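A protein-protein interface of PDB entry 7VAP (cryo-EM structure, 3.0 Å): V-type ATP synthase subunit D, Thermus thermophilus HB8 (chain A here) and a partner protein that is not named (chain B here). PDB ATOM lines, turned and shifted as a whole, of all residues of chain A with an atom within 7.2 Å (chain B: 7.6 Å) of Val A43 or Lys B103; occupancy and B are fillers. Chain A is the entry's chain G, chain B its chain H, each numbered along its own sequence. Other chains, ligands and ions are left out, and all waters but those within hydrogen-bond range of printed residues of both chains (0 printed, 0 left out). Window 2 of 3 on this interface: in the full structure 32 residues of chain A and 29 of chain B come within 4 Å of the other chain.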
ATOM      1  N   GLU A  38      19.909 -21.855 -26.597  1.00  0.00           N
ATOM      2  CA  GLU A  38      19.925 -22.789 -27.724  1.00  0.00           C
ATOM      3  C   GLU A  38      21.276 -23.496 -27.848  1.00  0.00           C
ATOM      4  O   GLU A  38      21.338 -24.673 -28.233  1.00  0.00           O
ATOM      5  CB  GLU A  38      19.569 -22.057 -29.018  1.00  0.00           C
ATOM      6  CG  GLU A  38      19.765 -22.885 -30.274  1.00  0.00           C
ATOM      7  CD  GLU A  38      18.866 -22.439 -31.404  1.00  0.00           C
ATOM      8  OE1 GLU A  38      18.325 -21.319 -31.315  1.00  0.00           O
ATOM      9  OE2 GLU A  38      18.699 -23.203 -32.377  1.00  0.00           O
ATOM     10  N   PHE A  39      22.364 -22.790 -27.534  1.00  0.00           N
ATOM     11  CA  PHE A  39      23.705 -23.339 -27.717  1.00  0.00           C
ATOM     12  C   PHE A  39      23.945 -24.534 -26.802  1.00  0.00           C
ATOM     13  O   PHE A  39      24.577 -25.519 -27.206  1.00  0.00           O
ATOM     14  CB  PHE A  39      24.735 -22.241 -27.460  1.00  0.00           C
ATOM     15  CG  PHE A  39      26.156 -22.680 -27.614  1.00  0.00           C
ATOM     16  CD1 PHE A  39      26.742 -22.704 -28.864  1.00  0.00           C
ATOM     17  CD2 PHE A  39      26.916 -23.039 -26.518  1.00  0.00           C
ATOM     18  CE1 PHE A  39      28.051 -23.088 -29.026  1.00  0.00           C
ATOM     19  CE2 PHE A  39      28.234 -23.428 -26.672  1.00  0.00           C
ATOM     20  CZ  PHE A  39      28.801 -23.451 -27.930  1.00  0.00           C
ATOM     21  N   PHE A  40      23.462 -24.459 -25.557  1.00  0.00           N
ATOM     22  CA  PHE A  40      23.606 -25.614 -24.669  1.00  0.00           C
ATOM     23  C   PHE A  40      22.710 -26.798 -25.022  1.00  0.00           C
ATOM     24  O   PHE A  40      22.856 -27.854 -24.400  1.00  0.00           O
ATOM     25  CB  PHE A  40      23.397 -25.237 -23.200  1.00  0.00           C
ATOM     26  CG  PHE A  40      24.476 -24.360 -22.638  1.00  0.00           C
ATOM     27  CD1 PHE A  40      25.666 -24.928 -22.228  1.00  0.00           C
ATOM     28  CD2 PHE A  40      24.309 -23.006 -22.472  1.00  0.00           C
ATOM     29  CE1 PHE A  40      26.682 -24.162 -21.695  1.00  0.00           C
ATOM     30  CE2 PHE A  40      25.329 -22.240 -21.927  1.00  0.00           C
ATOM     31  CZ  PHE A  40      26.510 -22.817 -21.544  1.00  0.00           C
ATOM     32  N   GLY A  41      21.799 -26.670 -25.979  1.00  0.00           N
ATOM     33  CA  GLY A  41      21.124 -27.854 -26.477  1.00  0.00           C
ATOM     34  C   GLY A  41      21.836 -28.391 -27.703  1.00  0.00           C
ATOM     35  O   GLY A  41      22.006 -29.608 -27.886  1.00  0.00           O
ATOM     36  N   LEU A  42      22.291 -27.459 -28.544  1.00  0.00           N
ATOM     37  CA  LEU A  42      23.020 -27.850 -29.744  1.00  0.00           C
ATOM     38  C   LEU A  42      24.322 -28.565 -29.399  1.00  0.00           C
ATOM     39  O   LEU A  42      24.753 -29.455 -30.141  1.00  0.00           O
ATOM     40  CB  LEU A  42      23.288 -26.626 -30.619  1.00  0.00           C
ATOM     41  CG  LEU A  42      23.599 -26.931 -32.083  1.00  0.00           C
ATOM     42  CD1 LEU A  42      22.525 -27.824 -32.676  1.00  0.00           C
ATOM     43  CD2 LEU A  42      23.719 -25.647 -32.877  1.00  0.00           C
ATOM     44  N   VAL A  43      24.949 -28.207 -28.276  1.00  0.00           N
ATOM     45  CA  VAL A  43      26.206 -28.851 -27.900  1.00  0.00           C
ATOM     46  C   VAL A  43      25.980 -30.321 -27.548  1.00  0.00           C
ATOM     47  O   VAL A  43      26.755 -31.194 -27.958  1.00  0.00           O
ATOM     48  CB  VAL A  43      26.886 -28.076 -26.754  1.00  0.00           C
ATOM     49  CG1 VAL A  43      26.016 -28.044 -25.512  1.00  0.00           C
ATOM     50  CG2 VAL A  43      28.243 -28.676 -26.434  1.00  0.00           C
ATOM     51  N   ARG A  44      24.917 -30.621 -26.796  1.00  0.00           N
ATOM     52  CA  ARG A  44      24.613 -32.015 -26.482  1.00  0.00           C
ATOM     53  C   ARG A  44      24.226 -32.787 -27.734  1.00  0.00           C
ATOM     54  O   ARG A  44      24.593 -33.961 -27.889  1.00  0.00           O
ATOM     55  CB  ARG A  44      23.496 -32.095 -25.442  1.00  0.00           C
ATOM     56  CG  ARG A  44      23.941 -31.775 -24.029  1.00  0.00           C
ATOM     57  CD  ARG A  44      22.742 -31.634 -23.112  1.00  0.00           C
ATOM     58  NE  ARG A  44      22.119 -30.323 -23.236  1.00  0.00           N
ATOM     59  CZ  ARG A  44      20.824 -30.093 -23.074  1.00  0.00           C
ATOM     60  NH1 ARG A  44      19.983 -31.070 -22.778  1.00  0.00           N
ATOM     61  NH2 ARG A  44      20.360 -28.855 -23.218  1.00  0.00           N
ATOM     62  N   GLU A  45      23.475 -32.150 -28.640  1.00  0.00           N
ATOM     63  CA  GLU A  45      23.158 -32.815 -29.900  1.00  0.00           C
ATOM     64  C   GLU A  45      24.427 -33.153 -30.678  1.00  0.00           C
ATOM     65  O   GLU A  45      24.562 -34.261 -31.215  1.00  0.00           O
ATOM     66  CB  GLU A  45      22.230 -31.940 -30.741  1.00  0.00           C
ATOM     67  CG  GLU A  45      21.820 -32.576 -32.055  1.00  0.00           C
ATOM     68  CD  GLU A  45      20.924 -33.783 -31.861  1.00  0.00           C
ATOM     69  OE1 GLU A  45      20.294 -33.894 -30.787  1.00  0.00           O
ATOM     70  OE2 GLU A  45      20.855 -34.625 -32.781  1.00  0.00           O
ATOM     71  N   ALA A  46      25.372 -32.212 -30.734  1.00  0.00           N
ATOM     72  CA  ALA A  46      26.630 -32.459 -31.429  1.00  0.00           C
ATOM     73  C   ALA A  46      27.417 -33.578 -30.766  1.00  0.00           C
ATOM     74  O   ALA A  46      28.044 -34.393 -31.450  1.00  0.00           O
ATOM     75  CB  ALA A  46      27.462 -31.178 -31.483  1.00  0.00           C
ATOM     76  N   MET A  47      27.406 -33.633 -29.434  1.00  0.00           N
ATOM     77  CA  MET A  47      28.129 -34.696 -28.739  1.00  0.00           C
ATOM     78  C   MET A  47      27.525 -36.065 -29.035  1.00  0.00           C
ATOM     79  O   MET A  47      28.255 -37.046 -29.244  1.00  0.00           O
ATOM     80  CB  MET A  47      28.143 -34.417 -27.238  1.00  0.00           C
ATOM     81  CG  MET A  47      29.354 -34.978 -26.516  1.00  0.00           C
ATOM     82  SD  MET A  47      29.581 -34.236 -24.890  1.00  0.00           S
ATOM     83  CE  MET A  47      28.153 -34.881 -24.021  1.00  0.00           C
ATOM     84  N   GLU A  48      26.193 -36.153 -29.054  1.00  0.00           N
ATOM     85  CA  GLU A  48      25.543 -37.414 -29.402  1.00  0.00           C
ATOM     86  C   GLU A  48      25.875 -37.826 -30.832  1.00  0.00           C
ATOM     87  O   GLU A  48      26.165 -39.001 -31.102  1.00  0.00           O
ATOM     88  CB  GLU A  48      24.032 -37.294 -29.216  1.00  0.00           C
ATOM     89  CG  GLU A  48      23.582 -37.310 -27.768  1.00  0.00           C
ATOM     90  CD  GLU A  48      23.671 -38.690 -27.154  1.00  0.00           C
ATOM     91  OE1 GLU A  48      23.430 -39.679 -27.878  1.00  0.00           O
ATOM     92  OE2 GLU A  48      23.981 -38.786 -25.948  1.00  0.00           O
ATOM     93  N   ALA A  49      25.841 -36.870 -31.763  1.00  0.00           N
ATOM     94  CA  ALA A  49      26.218 -37.179 -33.137  1.00  0.00           C
ATOM     95  C   ALA A  49      27.665 -37.649 -33.213  1.00  0.00           C
ATOM     96  O   ALA A  49      27.990 -38.565 -33.976  1.00  0.00           O
ATOM     97  CB  ALA A  49      25.995 -35.961 -34.032  1.00  0.00           C
ATOM     98  N   THR A 143      25.787 -30.749 -37.873  1.00  0.00           N
ATOM     99  CA  THR A 143      25.612 -30.223 -36.524  1.00  0.00           C
ATOM    100  C   THR A 143      26.739 -29.264 -36.152  1.00  0.00           C
ATOM    101  O   THR A 143      26.501 -28.231 -35.511  1.00  0.00           O
ATOM    102  CB  THR A 143      25.528 -31.373 -35.523  1.00  0.00           C
ATOM    103  OG1 THR A 143      24.658 -32.388 -36.040  1.00  0.00           O
ATOM    104  CG2 THR A 143      24.974 -30.878 -34.202  1.00  0.00           C
ATOM    105  N   LEU A 147      26.680 -25.368 -34.838  1.00  0.00           N
ATOM    106  CA  LEU A 147      27.258 -25.010 -33.547  1.00  0.00           C
ATOM    107  C   LEU A 147      28.240 -23.853 -33.687  1.00  0.00           C
ATOM    108  O   LEU A 147      28.236 -22.921 -32.874  1.00  0.00           O
ATOM    109  CB  LEU A 147      27.947 -26.224 -32.926  1.00  0.00           C
ATOM    110  CG  LEU A 147      28.272 -26.117 -31.435  1.00  0.00           C
ATOM    111  CD1 LEU A 147      27.030 -26.365 -30.596  1.00  0.00           C
ATOM    112  CD2 LEU A 147      29.382 -27.083 -31.052  1.00  0.00           C
ATOM    113  N   GLU B  87      33.754 -36.137 -24.834  1.00  0.00           N
ATOM    114  CA  GLU B  87      33.495 -35.081 -23.862  1.00  0.00           C
ATOM    115  C   GLU B  87      34.602 -34.034 -23.879  1.00  0.00           C
ATOM    116  O   GLU B  87      34.325 -32.832 -23.811  1.00  0.00           O
ATOM    117  CB  GLU B  87      33.342 -35.681 -22.464  1.00  0.00           C
ATOM    118  CG  GLU B  87      33.248 -34.656 -21.340  1.00  0.00           C
ATOM    119  CD  GLU B  87      34.603 -34.301 -20.752  1.00  0.00           C
ATOM    120  OE1 GLU B  87      35.531 -35.130 -20.856  1.00  0.00           O
ATOM    121  OE2 GLU B  87      34.739 -33.194 -20.189  1.00  0.00           O
ATOM    122  N   MET B  90      34.366 -31.938 -27.103  1.00  0.00           N
ATOM    123  CA  MET B  90      33.227 -31.032 -26.998  1.00  0.00           C
ATOM    124  C   MET B  90      33.518 -29.886 -26.036  1.00  0.00           C
ATOM    125  O   MET B  90      33.142 -28.739 -26.297  1.00  0.00           O
ATOM    126  CB  MET B  90      31.987 -31.807 -26.558  1.00  0.00           C
ATOM    127  CG  MET B  90      30.679 -31.247 -27.084  1.00  0.00           C
ATOM    128  SD  MET B  90      30.662 -31.038 -28.873  1.00  0.00           S
ATOM    129  CE  MET B  90      31.043 -32.700 -29.421  1.00  0.00           C
ATOM    130  N   ARG B  91      34.187 -30.178 -24.920  1.00  0.00           N
ATOM    131  CA  ARG B  91      34.576 -29.126 -23.987  1.00  0.00           C
ATOM    132  C   ARG B  91      35.552 -28.152 -24.631  1.00  0.00           C
ATOM    133  O   ARG B  91      35.464 -26.936 -24.420  1.00  0.00           O
ATOM    134  CB  ARG B  91      35.186 -29.743 -22.730  1.00  0.00           C
ATOM    135  CG  ARG B  91      35.767 -28.734 -21.761  1.00  0.00           C
ATOM    136  CD  ARG B  91      36.400 -29.421 -20.565  1.00  0.00           C
ATOM    137  NE  ARG B  91      35.434 -30.218 -19.818  1.00  0.00           N
ATOM    138  CZ  ARG B  91      34.559 -29.721 -18.956  1.00  0.00           C
ATOM    139  NH1 ARG B  91      34.504 -28.425 -18.697  1.00  0.00           N
ATOM    140  NH2 ARG B  91      33.716 -30.544 -18.338  1.00  0.00           N
ATOM    141  N   LEU B  93      35.715 -27.461 -27.828  1.00  0.00           N
ATOM    142  CA  LEU B  93      34.912 -26.643 -28.734  1.00  0.00           C
ATOM    143  C   LEU B  93      34.127 -25.579 -27.974  1.00  0.00           C
ATOM    144  O   LEU B  93      33.983 -24.446 -28.448  1.00  0.00           O
ATOM    145  CB  LEU B  93      33.968 -27.526 -29.551  1.00  0.00           C
ATOM    146  CG  LEU B  93      34.473 -27.965 -30.926  1.00  0.00           C
ATOM    147  CD1 LEU B  93      34.588 -26.764 -31.853  1.00  0.00           C
ATOM    148  CD2 LEU B  93      35.806 -28.676 -30.814  1.00  0.00           C
ATOM    149  N   VAL B  94      33.602 -25.930 -26.799  1.00  0.00           N
ATOM    150  CA  VAL B  94      32.899 -24.949 -25.975  1.00  0.00           C
ATOM    151  C   VAL B  94      33.841 -23.823 -25.573  1.00  0.00           C
ATOM    152  O   VAL B  94      33.468 -22.643 -25.582  1.00  0.00           O
ATOM    153  CB  VAL B  94      32.269 -25.631 -24.745  1.00  0.00           C
ATOM    154  CG1 VAL B  94      31.791 -24.594 -23.744  1.00  0.00           C
ATOM    155  CG2 VAL B  94      31.115 -26.520 -25.170  1.00  0.00           C
ATOM    156  N   THR B  97      34.346 -21.572 -28.497  1.00  0.00           N
ATOM    157  CA  THR B  97      33.185 -20.756 -28.834  1.00  0.00           C
ATOM    158  C   THR B  97      32.955 -19.641 -27.816  1.00  0.00           C
ATOM    159  O   THR B  97      32.901 -18.461 -28.176  1.00  0.00           O
ATOM    160  CB  THR B  97      31.939 -21.638 -28.950  1.00  0.00           C
ATOM    161  OG1 THR B  97      31.822 -22.460 -27.783  1.00  0.00           O
ATOM    162  CG2 THR B  97      32.026 -22.523 -30.183  1.00  0.00           C
ATOM    163  N   PHE B 100      34.375 -19.918 -21.606  1.00  0.00           N
ATOM    164  CA  PHE B 100      34.190 -20.105 -20.170  1.00  0.00           C
ATOM    165  C   PHE B 100      34.773 -21.427 -19.689  1.00  0.00           C
ATOM    166  O   PHE B 100      35.259 -21.509 -18.554  1.00  0.00           O
ATOM    167  CB  PHE B 100      32.709 -20.007 -19.809  1.00  0.00           C
ATOM    168  CG  PHE B 100      32.237 -18.601 -19.579  1.00  0.00           C
ATOM    169  CD1 PHE B 100      33.078 -17.528 -19.819  1.00  0.00           C
ATOM    170  CD2 PHE B 100      30.955 -18.351 -19.122  1.00  0.00           C
ATOM    171  CE1 PHE B 100      32.652 -16.234 -19.609  1.00  0.00           C
ATOM    172  CE2 PHE B 100      30.521 -17.057 -18.910  1.00  0.00           C
ATOM    173  CZ  PHE B 100      31.371 -15.997 -19.154  1.00  0.00           C
ATOM    174  N   ASP B 101      34.737 -22.463 -20.528  1.00  0.00           N
ATOM    175  CA  ASP B 101      35.237 -23.793 -20.178  1.00  0.00           C
ATOM    176  C   ASP B 101      34.582 -24.291 -18.888  1.00  0.00           C
ATOM    177  O   ASP B 101      35.245 -24.666 -17.918  1.00  0.00           O
ATOM    178  CB  ASP B 101      36.767 -23.791 -20.069  1.00  0.00           C
ATOM    179  CG  ASP B 101      37.351 -25.188 -19.964  1.00  0.00           C
ATOM    180  OD1 ASP B 101      36.579 -26.167 -20.025  1.00  0.00           O
ATOM    181  OD2 ASP B 101      38.587 -25.308 -19.825  1.00  0.00           O
ATOM    182  N   ILE B 102      33.252 -24.273 -18.891  1.00  0.00           N
ATOM    183  CA  ILE B 102      32.446 -24.682 -17.746  1.00  0.00           C
ATOM    184  C   ILE B 102      31.290 -25.512 -18.290  1.00  0.00           C
ATOM    185  O   ILE B 102      30.368 -24.973 -18.912  1.00  0.00           O
ATOM    186  CB  ILE B 102      31.936 -23.487 -16.934  1.00  0.00           C
ATOM    187  CG1 ILE B 102      33.104 -22.758 -16.264  1.00  0.00           C
ATOM    188  CG2 ILE B 102      30.933 -23.940 -15.893  1.00  0.00           C
ATOM    189  CD1 ILE B 102      32.703 -21.498 -15.529  1.00  0.00           C
ATOM    190  N   LYS B 103      31.337 -26.823 -18.064  1.00  0.00           N
ATOM    191  CA  LYS B 103      30.266 -27.711 -18.493  1.00  0.00           C
ATOM    192  C   LYS B 103      30.358 -29.012 -17.711  1.00  0.00           C
ATOM    193  O   LYS B 103      31.453 -29.516 -17.446  1.00  0.00           O
ATOM    194  CB  LYS B 103      30.331 -27.990 -19.998  1.00  0.00           C
ATOM    195  CG  LYS B 103      29.131 -28.755 -20.539  1.00  0.00           C
ATOM    196  CD  LYS B 103      29.204 -28.902 -22.050  1.00  0.00           C
ATOM    197  CE  LYS B 103      27.982 -29.628 -22.591  1.00  0.00           C
ATOM    198  NZ  LYS B 103      27.915 -31.033 -22.103  1.00  0.00           N
ATOM    199  N   LEU B 104      29.194 -29.548 -17.353  1.00  0.00           N
ATOM    200  CA  LEU B 104      29.107 -30.818 -16.636  1.00  0.00           C
ATOM    201  C   LEU B 104      27.677 -31.352 -16.642  1.00  0.00           C
ATOM    202  O   LEU B 104      27.150 -31.736 -17.687  1.00  0.00           O
ATOM    203  CB  LEU B 104      29.620 -30.660 -15.199  1.00  0.00           C
ATOM    204  CG  LEU B 104      28.968 -29.629 -14.272  1.00  0.00           C
ATOM    205  CD1 LEU B 104      27.757 -30.192 -13.537  1.00  0.00           C
ATOM    206  CD2 LEU B 104      29.996 -29.102 -13.289  1.00  0.00           C
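The guanidinium group (NH2) of Arg B91 lies within hydrogen-bond range of the backbone carbonyl oxygen (O) of Lys B103, at 2.6 Å. The backbone carbonyl oxygen (O) of Leu B93 lies within hydrogen-bond range of the side-chain hydroxyl (OG1) of Thr B97 (3.0 Å). O of Val B94 is in hydrogen-bond range of OG1 of Thr B97 (2.8 Å).
CZ of Phe A39 touches OG1 of Thr B97 (3.2 Å). Met B90 touches Val A43 (CG to CG2, 3.6 Å). Val B94 touches Val A43. CG1 of Val A43 touches CE of Lys B103, 3.9 Å away. Ala A46 touches Met B90 (C to CE, 3.97 Å). CE of Met B90 touches CA of Met A47, 3.6 Å away.
Val A43 touches just these residues of chain B: Met B90 (3.6 Å), Val B94 (3.8 Å) and Lys B103 (3.9 Å). Leu A147 touches none of the printed residues of chain B. Printed residues of chain A within 4 Å of Val B94: Val A43 (3.8 Å). Of the printed residues of chain A, Thr B97 touches Phe A39 (3.2 Å). Phe B100 touches none of the printed residues of chain A. The nearest residue of chain B that does not touch Val A43 is Arg B91 (6.3 Å).
Printed residues of chain A that touch a printed residue of chain B: Phe A39, Val A43, Ala A46 and Met A47. Hydrophobic or aromatic side chains of chain B within 4 Å of the printed part of chain A: Met B90 and Val B94. Among the printed residues, no Asp or Glu carboxylate lies within 4 Å of a Lys or Arg side-chain nitrogen of the other chain.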
